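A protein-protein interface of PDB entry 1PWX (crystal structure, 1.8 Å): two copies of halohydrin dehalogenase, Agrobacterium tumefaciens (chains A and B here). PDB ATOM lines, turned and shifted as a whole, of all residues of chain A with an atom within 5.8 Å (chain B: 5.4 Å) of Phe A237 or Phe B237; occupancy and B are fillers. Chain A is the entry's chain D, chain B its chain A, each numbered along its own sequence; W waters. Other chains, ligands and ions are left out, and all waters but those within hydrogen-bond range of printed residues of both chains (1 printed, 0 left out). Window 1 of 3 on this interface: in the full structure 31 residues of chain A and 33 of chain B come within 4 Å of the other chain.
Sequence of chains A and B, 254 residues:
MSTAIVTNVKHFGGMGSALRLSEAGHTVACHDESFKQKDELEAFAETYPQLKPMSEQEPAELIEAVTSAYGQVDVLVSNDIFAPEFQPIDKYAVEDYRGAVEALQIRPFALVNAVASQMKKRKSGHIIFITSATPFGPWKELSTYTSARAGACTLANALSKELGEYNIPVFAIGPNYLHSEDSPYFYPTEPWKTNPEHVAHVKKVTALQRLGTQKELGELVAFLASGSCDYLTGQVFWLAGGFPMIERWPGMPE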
ATOM      1  N   PHE A 171     -17.117  21.659  12.049  1.00  0.00           N
ATOM      2  CA  PHE A 171     -15.790  21.417  12.606  1.00  0.00           C
ATOM      3  C   PHE A 171     -15.225  22.646  13.285  1.00  0.00           C
ATOM      4  O   PHE A 171     -15.556  23.768  12.921  1.00  0.00           O
ATOM      5  CB  PHE A 171     -14.831  20.964  11.503  1.00  0.00           C
ATOM      6  CG  PHE A 171     -15.333  19.791  10.711  1.00  0.00           C
ATOM      7  CD1 PHE A 171     -15.905  19.976   9.455  1.00  0.00           C
ATOM      8  CD2 PHE A 171     -15.248  18.499  11.223  1.00  0.00           C
ATOM      9  CE1 PHE A 171     -16.384  18.890   8.719  1.00  0.00           C
ATOM     10  CE2 PHE A 171     -15.722  17.415  10.500  1.00  0.00           C
ATOM     11  CZ  PHE A 171     -16.289  17.609   9.249  1.00  0.00           C
ATOM     12  N   ALA A 172     -14.374  22.415  14.273  1.00  0.00           N
ATOM     13  CA  ALA A 172     -13.722  23.493  15.004  1.00  0.00           C
ATOM     14  C   ALA A 172     -12.205  23.341  14.837  1.00  0.00           C
ATOM     15  O   ALA A 172     -11.641  22.287  15.158  1.00  0.00           O
ATOM     16  CB  ALA A 172     -14.103  23.431  16.494  1.00  0.00           C
ATOM     17  N   ILE A 173     -11.554  24.373  14.301  1.00  0.00           N
ATOM     18  CA  ILE A 173     -10.105  24.338  14.136  1.00  0.00           C
ATOM     19  C   ILE A 173      -9.510  25.279  15.159  1.00  0.00           C
ATOM     20  O   ILE A 173      -9.686  26.497  15.079  1.00  0.00           O
ATOM     21  CB  ILE A 173      -9.645  24.768  12.708  1.00  0.00           C
ATOM     22  CG1 ILE A 173      -9.923  23.647  11.701  1.00  0.00           C
ATOM     23  CG2 ILE A 173      -8.138  25.064  12.695  1.00  0.00           C
ATOM     24  CD1 ILE A 173     -11.373  23.382  11.463  1.00  0.00           C
ATOM     25  N   GLY A 174      -8.826  24.695  16.137  1.00  0.00           N
ATOM     26  CA  GLY A 174      -8.198  25.469  17.188  1.00  0.00           C
ATOM     27  C   GLY A 174      -6.695  25.501  17.003  1.00  0.00           C
ATOM     28  O   GLY A 174      -5.983  24.631  17.499  1.00  0.00           O
ATOM     29  N   PRO A 175      -6.171  26.499  16.285  1.00  0.00           N
ATOM     30  CA  PRO A 175      -4.717  26.481  16.135  1.00  0.00           C
ATOM     31  C   PRO A 175      -4.035  27.387  17.148  1.00  0.00           C
ATOM     32  O   PRO A 175      -4.691  28.061  17.952  1.00  0.00           O
ATOM     33  CB  PRO A 175      -4.532  26.984  14.713  1.00  0.00           C
ATOM     34  CG  PRO A 175      -5.573  28.074  14.656  1.00  0.00           C
ATOM     35  CD  PRO A 175      -6.790  27.470  15.361  1.00  0.00           C
ATOM     36  N   LEU A 220      -6.404  21.909   5.496  1.00  0.00           N
ATOM     37  CA  LEU A 220      -7.386  21.336   6.398  1.00  0.00           C
ATOM     38  C   LEU A 220      -8.759  21.943   6.173  1.00  0.00           C
ATOM     39  O   LEU A 220      -9.764  21.231   6.186  1.00  0.00           O
ATOM     40  CB  LEU A 220      -6.984  21.560   7.850  1.00  0.00           C
ATOM     41  CG  LEU A 220      -8.066  21.197   8.881  1.00  0.00           C
ATOM     42  CD1 LEU A 220      -8.401  19.710   8.774  1.00  0.00           C
ATOM     43  CD2 LEU A 220      -7.584  21.567  10.281  1.00  0.00           C
ATOM     44  N   LEU A 224     -11.907  19.473   4.832  1.00  0.00           N
ATOM     45  CA  LEU A 224     -13.188  19.318   5.511  1.00  0.00           C
ATOM     46  C   LEU A 224     -14.359  19.830   4.656  1.00  0.00           C
ATOM     47  O   LEU A 224     -15.405  19.189   4.582  1.00  0.00           O
ATOM     48  CB  LEU A 224     -13.153  20.052   6.866  1.00  0.00           C
ATOM     49  CG  LEU A 224     -12.081  19.631   7.885  1.00  0.00           C
ATOM     50  CD1 LEU A 224     -12.206  20.498   9.129  1.00  0.00           C
ATOM     51  CD2 LEU A 224     -12.226  18.141   8.229  1.00  0.00           C
ATOM     52  N   LEU A 232     -16.174  13.045  10.177  1.00  0.00           N
ATOM     53  CA  LEU A 232     -15.461  13.617  11.326  1.00  0.00           C
ATOM     54  C   LEU A 232     -16.276  14.748  11.943  1.00  0.00           C
ATOM     55  O   LEU A 232     -15.734  15.570  12.700  1.00  0.00           O
ATOM     56  CB  LEU A 232     -14.106  14.206  10.915  1.00  0.00           C
ATOM     57  CG  LEU A 232     -12.866  13.352  10.683  1.00  0.00           C
ATOM     58  CD1 LEU A 232     -11.763  14.247  10.104  1.00  0.00           C
ATOM     59  CD2 LEU A 232     -12.408  12.724  11.982  1.00  0.00           C
ATOM     60  N   GLN A 235     -15.773  17.334  15.178  1.00  0.00           N
ATOM     61  CA  GLN A 235     -14.377  17.283  15.578  1.00  0.00           C
ATOM     62  C   GLN A 235     -13.779  18.665  15.821  1.00  0.00           C
ATOM     63  O   GLN A 235     -14.140  19.642  15.159  1.00  0.00           O
ATOM     64  CB  GLN A 235     -13.550  16.582  14.500  1.00  0.00           C
ATOM     65  CG  GLN A 235     -12.035  16.622  14.708  1.00  0.00           C
ATOM     66  CD  GLN A 235     -11.546  15.528  15.640  1.00  0.00           C
ATOM     67  OE1 GLN A 235     -11.972  14.378  15.538  1.00  0.00           O
ATOM     68  NE2 GLN A 235     -10.634  15.879  16.540  1.00  0.00           N
ATOM     69  N   VAL A 236     -12.890  18.737  16.805  1.00  0.00           N
ATOM     70  CA  VAL A 236     -12.165  19.968  17.084  1.00  0.00           C
ATOM     71  C   VAL A 236     -10.741  19.552  16.734  1.00  0.00           C
ATOM     72  O   VAL A 236     -10.294  18.471  17.134  1.00  0.00           O
ATOM     73  CB  VAL A 236     -12.241  20.395  18.582  1.00  0.00           C
ATOM     74  CG1 VAL A 236     -11.329  21.606  18.828  1.00  0.00           C
ATOM     75  CG2 VAL A 236     -13.673  20.766  18.945  1.00  0.00           C
ATOM     76  N   PHE A 237     -10.041  20.380  15.965  1.00  0.00           N
ATOM     77  CA  PHE A 237      -8.669  20.073  15.563  1.00  0.00           C
ATOM     78  C   PHE A 237      -7.697  20.962  16.322  1.00  0.00           C
ATOM     79  O   PHE A 237      -7.876  22.173  16.358  1.00  0.00           O
ATOM     80  CB  PHE A 237      -8.489  20.317  14.054  1.00  0.00           C
ATOM     81  CG  PHE A 237      -9.415  19.507  13.188  1.00  0.00           C
ATOM     82  CD1 PHE A 237      -8.997  18.302  12.638  1.00  0.00           C
ATOM     83  CD2 PHE A 237     -10.730  19.924  12.970  1.00  0.00           C
ATOM     84  CE1 PHE A 237      -9.883  17.521  11.886  1.00  0.00           C
ATOM     85  CE2 PHE A 237     -11.610  19.153  12.230  1.00  0.00           C
ATOM     86  CZ  PHE A 237     -11.189  17.949  11.689  1.00  0.00           C
ATOM     87  N   TRP A 238      -6.682  20.375  16.950  1.00  0.00           N
ATOM     88  CA  TRP A 238      -5.683  21.189  17.658  1.00  0.00           C
ATOM     89  C   TRP A 238      -4.536  21.422  16.675  1.00  0.00           C
ATOM     90  O   TRP A 238      -3.589  20.640  16.617  1.00  0.00           O
ATOM     91  CB  TRP A 238      -5.140  20.482  18.908  1.00  0.00           C
ATOM     92  CG  TRP A 238      -6.159  20.165  19.984  1.00  0.00           C
ATOM     93  CD1 TRP A 238      -6.404  18.941  20.526  1.00  0.00           C
ATOM     94  CD2 TRP A 238      -7.009  21.088  20.688  1.00  0.00           C
ATOM     95  NE1 TRP A 238      -7.339  19.037  21.521  1.00  0.00           N
ATOM     96  CE2 TRP A 238      -7.730  20.345  21.642  1.00  0.00           C
ATOM     97  CE3 TRP A 238      -7.226  22.469  20.607  1.00  0.00           C
ATOM     98  CZ2 TRP A 238      -8.661  20.933  22.516  1.00  0.00           C
ATOM     99  CZ3 TRP A 238      -8.157  23.056  21.480  1.00  0.00           C
ATOM    100  CH2 TRP A 238      -8.859  22.283  22.420  1.00  0.00           C
ATOM    101  N   LEU A 239      -4.642  22.484  15.881  1.00  0.00           N
ATOM    102  CA  LEU A 239      -3.612  22.804  14.903  1.00  0.00           C
ATOM    103  C   LEU A 239      -2.550  23.592  15.666  1.00  0.00           C
ATOM    104  O   LEU A 239      -2.345  24.782  15.423  1.00  0.00           O
ATOM    105  CB  LEU A 239      -4.222  23.638  13.760  1.00  0.00           C
ATOM    106  CG  LEU A 239      -3.525  23.862  12.404  1.00  0.00           C
ATOM    107  CD1 LEU A 239      -2.390  24.842  12.542  1.00  0.00           C
ATOM    108  CD2 LEU A 239      -3.032  22.542  11.841  1.00  0.00           C
ATOM    109  N   PHE B 171      -0.402  10.453  14.587  1.00  0.00           N
ATOM    110  CA  PHE B 171      -1.821  10.648  14.822  1.00  0.00           C
ATOM    111  C   PHE B 171      -2.501   9.345  15.194  1.00  0.00           C
ATOM    112  O   PHE B 171      -1.904   8.271  15.168  1.00  0.00           O
ATOM    113  CB  PHE B 171      -2.516  11.190  13.560  1.00  0.00           C
ATOM    114  CG  PHE B 171      -1.697  12.189  12.782  1.00  0.00           C
ATOM    115  CD1 PHE B 171      -0.845  11.765  11.769  1.00  0.00           C
ATOM    116  CD2 PHE B 171      -1.792  13.553  13.059  1.00  0.00           C
ATOM    117  CE1 PHE B 171      -0.104  12.683  11.043  1.00  0.00           C
ATOM    118  CE2 PHE B 171      -1.051  14.481  12.335  1.00  0.00           C
ATOM    119  CZ  PHE B 171      -0.209  14.050  11.330  1.00  0.00           C
ATOM    120  N   ALA B 172      -3.769   9.469  15.547  1.00  0.00           N
ATOM    121  CA  ALA B 172      -4.599   8.325  15.869  1.00  0.00           C
ATOM    122  C   ALA B 172      -5.979   8.648  15.313  1.00  0.00           C
ATOM    123  O   ALA B 172      -6.440   9.779  15.392  1.00  0.00           O
ATOM    124  CB  ALA B 172      -4.657   8.102  17.392  1.00  0.00           C
ATOM    125  N   ILE B 173      -6.616   7.659  14.713  1.00  0.00           N
ATOM    126  CA  ILE B 173      -7.954   7.841  14.169  1.00  0.00           C
ATOM    127  C   ILE B 173      -8.862   6.881  14.936  1.00  0.00           C
ATOM    128  O   ILE B 173      -8.681   5.665  14.872  1.00  0.00           O
ATOM    129  CB  ILE B 173      -7.990   7.516  12.665  1.00  0.00           C
ATOM    130  CG1 ILE B 173      -6.935   8.352  11.931  1.00  0.00           C
ATOM    131  CG2 ILE B 173      -9.383   7.792  12.105  1.00  0.00           C
ATOM    132  CD1 ILE B 173      -6.771   7.990  10.483  1.00  0.00           C
ATOM    133  N   GLY B 174      -9.823   7.436  15.672  1.00  0.00           N
ATOM    134  CA  GLY B 174     -10.732   6.610  16.444  1.00  0.00           C
ATOM    135  C   GLY B 174     -12.072   6.424  15.757  1.00  0.00           C
ATOM    136  O   GLY B 174     -12.970   7.231  15.958  1.00  0.00           O
ATOM    137  N   PRO B 175     -12.241   5.369  14.940  1.00  0.00           N
ATOM    138  CA  PRO B 175     -13.530   5.181  14.268  1.00  0.00           C
ATOM    139  C   PRO B 175     -14.623   4.581  15.165  1.00  0.00           C
ATOM    140  O   PRO B 175     -14.353   4.090  16.267  1.00  0.00           O
ATOM    141  CB  PRO B 175     -13.179   4.259  13.090  1.00  0.00           C
ATOM    142  CG  PRO B 175     -11.645   4.334  12.986  1.00  0.00           C
ATOM    143  CD  PRO B 175     -11.235   4.433  14.408  1.00  0.00           C
ATOM    144  N   LEU B 220      -8.784  10.758   5.032  1.00  0.00           N
ATOM    145  CA  LEU B 220      -8.077  11.309   6.181  1.00  0.00           C
ATOM    146  C   LEU B 220      -6.675  10.725   6.263  1.00  0.00           C
ATOM    147  O   LEU B 220      -5.702  11.462   6.240  1.00  0.00           O
ATOM    148  CB  LEU B 220      -8.838  11.023   7.477  1.00  0.00           C
ATOM    149  CG  LEU B 220      -8.144  11.546   8.739  1.00  0.00           C
ATOM    150  CD1 LEU B 220      -8.155  13.061   8.733  1.00  0.00           C
ATOM    151  CD2 LEU B 220      -8.853  11.012   9.963  1.00  0.00           C
ATOM    152  N   LEU B 224      -3.544  12.984   6.029  1.00  0.00           N
ATOM    153  CA  LEU B 224      -2.527  13.153   7.056  1.00  0.00           C
ATOM    154  C   LEU B 224      -1.171  12.686   6.524  1.00  0.00           C
ATOM    155  O   LEU B 224      -0.143  13.342   6.742  1.00  0.00           O
ATOM    156  CB  LEU B 224      -2.918  12.360   8.305  1.00  0.00           C
ATOM    157  CG  LEU B 224      -4.335  12.610   8.841  1.00  0.00           C
ATOM    158  CD1 LEU B 224      -4.635  11.650   9.991  1.00  0.00           C
ATOM    159  CD2 LEU B 224      -4.472  14.064   9.282  1.00  0.00           C
ATOM    160  N   LEU B 232      -0.987  19.007  12.810  1.00  0.00           N
ATOM    161  CA  LEU B 232      -2.042  18.401  13.629  1.00  0.00           C
ATOM    162  C   LEU B 232      -1.451  17.318  14.527  1.00  0.00           C
ATOM    163  O   LEU B 232      -2.128  16.798  15.428  1.00  0.00           O
ATOM    164  CB  LEU B 232      -3.137  17.766  12.762  1.00  0.00           C
ATOM    165  CG  LEU B 232      -4.145  18.701  12.094  1.00  0.00           C
ATOM    166  CD1 LEU B 232      -5.265  17.881  11.503  1.00  0.00           C
ATOM    167  CD2 LEU B 232      -4.709  19.684  13.106  1.00  0.00           C
ATOM    168  N   GLN B 235      -2.721  14.613  17.326  1.00  0.00           N
ATOM    169  CA  GLN B 235      -4.180  14.648  17.266  1.00  0.00           C
ATOM    170  C   GLN B 235      -4.883  13.303  17.158  1.00  0.00           C
ATOM    171  O   GLN B 235      -4.444  12.407  16.437  1.00  0.00           O
ATOM    172  CB  GLN B 235      -4.632  15.515  16.087  1.00  0.00           C
ATOM    173  CG  GLN B 235      -6.140  15.594  15.897  1.00  0.00           C
ATOM    174  CD  GLN B 235      -6.769  16.763  16.639  1.00  0.00           C
ATOM    175  OE1 GLN B 235      -6.357  17.914  16.471  1.00  0.00           O
ATOM    176  NE2 GLN B 235      -7.786  16.475  17.455  1.00  0.00           N
ATOM    177  N   VAL B 236      -5.992  13.186  17.884  1.00  0.00           N
ATOM    178  CA  VAL B 236      -6.831  11.994  17.856  1.00  0.00           C
ATOM    179  C   VAL B 236      -8.116  12.338  17.099  1.00  0.00           C
ATOM    180  O   VAL B 236      -8.908  13.162  17.553  1.00  0.00           O
ATOM    181  CB  VAL B 236      -7.255  11.549  19.251  1.00  0.00           C
ATOM    182  CG1 VAL B 236      -8.329  10.461  19.133  1.00  0.00           C
ATOM    183  CG2 VAL B 236      -6.049  11.045  20.025  1.00  0.00           C
ATOM    184  N   PHE B 237      -8.329  11.704  15.959  1.00  0.00           N
ATOM    185  CA  PHE B 237      -9.522  11.979  15.186  1.00  0.00           C
ATOM    186  C   PHE B 237     -10.691  11.089  15.607  1.00  0.00           C
ATOM    187  O   PHE B 237     -10.515   9.903  15.886  1.00  0.00           O
ATOM    188  CB  PHE B 237      -9.214  11.811  13.702  1.00  0.00           C
ATOM    189  CG  PHE B 237      -8.135  12.734  13.208  1.00  0.00           C
ATOM    190  CD1 PHE B 237      -8.457  13.897  12.522  1.00  0.00           C
ATOM    191  CD2 PHE B 237      -6.794  12.442  13.439  1.00  0.00           C
ATOM    192  CE1 PHE B 237      -7.466  14.757  12.069  1.00  0.00           C
ATOM    193  CE2 PHE B 237      -5.786  13.297  12.991  1.00  0.00           C
ATOM    194  CZ  PHE B 237      -6.124  14.459  12.303  1.00  0.00           C
ATOM    195  N   TRP B 238     -11.877  11.687  15.681  1.00  0.00           N
ATOM    196  CA  TRP B 238     -13.091  10.969  16.054  1.00  0.00           C
ATOM    197  C   TRP B 238     -13.901  10.785  14.790  1.00  0.00           C
ATOM    198  O   TRP B 238     -14.666  11.667  14.394  1.00  0.00           O
ATOM    199  CB  TRP B 238     -13.898  11.764  17.081  1.00  0.00           C
ATOM    200  CG  TRP B 238     -13.088  12.127  18.292  1.00  0.00           C
ATOM    201  CD1 TRP B 238     -12.807  13.387  18.745  1.00  0.00           C
ATOM    202  CD2 TRP B 238     -12.412  11.218  19.181  1.00  0.00           C
ATOM    203  NE1 TRP B 238     -11.997  13.320  19.851  1.00  0.00           N
ATOM    204  CE2 TRP B 238     -11.738  12.005  20.145  1.00  0.00           C
ATOM    205  CE3 TRP B 238     -12.309   9.816  19.252  1.00  0.00           C
ATOM    206  CZ2 TRP B 238     -10.968  11.440  21.175  1.00  0.00           C
ATOM    207  CZ3 TRP B 238     -11.540   9.249  20.275  1.00  0.00           C
ATOM    208  CH2 TRP B 238     -10.879  10.071  21.226  1.00  0.00           C
ATOM    209  N   LEU B 239     -13.707   9.635  14.155  1.00  0.00           N
ATOM    210  CA  LEU B 239     -14.395   9.306  12.918  1.00  0.00           C
ATOM    211  C   LEU B 239     -15.653   8.504  13.243  1.00  0.00           C
ATOM    212  O   LEU B 239     -15.929   7.487  12.603  1.00  0.00           O
ATOM    213  CB  LEU B 239     -13.482   8.464  12.032  1.00  0.00           C
ATOM    214  CG  LEU B 239     -13.204   8.816  10.566  1.00  0.00           C
ATOM    215  CD1 LEU B 239     -12.819   7.521   9.853  1.00  0.00           C
ATOM    216  CD2 LEU B 239     -14.396   9.445   9.892  1.00  0.00           C
HETATM  217  O   HOH W   1      -9.867  16.375  19.167  1.00  0.00           O
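The side-chain amide oxygen of Gln B235 is in hydrogen-bond range of the backbone NH of Trp A238 (2.5 Å). The side-chain amide nitrogen (NE2) of Gln B235 lies close to the side-chain amide nitrogen (NE2) of Gln A235. The side-chain amide nitrogen (NE2) of Gln B235 is in hydrogen-bond range of the backbone carbonyl oxygen (O) of Val A236 (3.2 Å). N of Trp B238 lies within hydrogen-bond range of OE1 of Gln A235, 2.7 Å away. O of Val B236 is in hydrogen-bond range of NE2 of Gln A235 (3.4 Å).
The backbone carbonyl oxygen (O) of Gly A174 is in hydrogen-bond range of the backbone NH (N) of Leu A239. The backbone NH (N) of Phe A237 sits at hydrogen-bond distance from the backbone carbonyl oxygen (O) of Ala A172 (2.6 Å). O of Ala B172 sits at hydrogen-bond distance from N of Phe B237 (2.8 Å). The backbone NH of Ala B172 lies within hydrogen-bond range of the backbone carbonyl oxygen of Gln B235. The backbone carbonyl oxygen of Phe B237 is in hydrogen-bond range of the backbone NH of Gly B174 (2.6 Å). The backbone NH of Leu B239 sits at hydrogen-bond distance from the backbone carbonyl oxygen of Gly B174 (3.1 Å).
Among the printed residues, pairs that only touch across the chains: Phe A237 with Gln B235, Gln A235 with Phe B237, Leu A232 with Trp B238, Leu A239 with Leu B232, Phe A237 with Phe B237, Leu A232 with Phe B237, Trp A238 with Leu B232, Phe A237 with Leu B232 and Leu A232 with Leu B239.
Of chain B, only Leu B232 (3.9 Å), Gln B235 (3.3 Å) and Phe B237 (3.7 Å) come within 4 Å of Phe A237. Phe B237 touches just these residues of chain A: Leu A232, Gln A235 and Phe A237. Of the printed residues of chain A, Leu B232 touches Phe A237, Trp A238 and Leu A239. Of the printed residues of chain B, Val A236 touches Gln B235. Of the printed residues of chain B, Gln A235 touches Gln B235 (3.1 Å), Val B236 (3.4 Å), Phe B237 (3.4 Å) and Trp B238 (2.7 Å). The nearest printed residue of chain B that does not touch Val A236 is Val B236 (5.5 Å).
Of the 13 printed residues of chain B, 6 touch a printed residue of chain A. Along chain B the printed residues that touch a printed residue of chain A span positions 232 to 239. Of the 13 printed residues of chain A, 6 touch a printed residue of chain B. Hydrophobic or aromatic side chains of chain A within 4 Å of the printed part of chain B: Leu A232, Phe A237, Trp A238 and Leu A239. Among the printed residues, no Asp or Glu carboxylate lies within 4 Å of a Lys or Arg side-chain nitrogen of the other chain.
Leu A232 touches Phe B237, and with the chains exchanged Phe A237 touches Leu B232. Leu A232 touches Leu B239, and with the chains exchanged Leu A239 touches Leu B232. Gln A235 touches its own counterpart, Gln B235. Gln A235 touches Trp B238, and with the chains exchanged Trp A238 touches Gln B235. Positions printed for both chains: 171, 172, 173, 174, 175, 220, 224, 232, 235, 236, 237, 238 and 239.
Water W1 lies within hydrogen-bond range of the side-chain amide nitrogen of Gln B235 (2.7 Å), the side-chain amide nitrogen of Gln A235 (2.8 Å) and the backbone carbonyl oxygen of Val A236 (3.0 Å).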
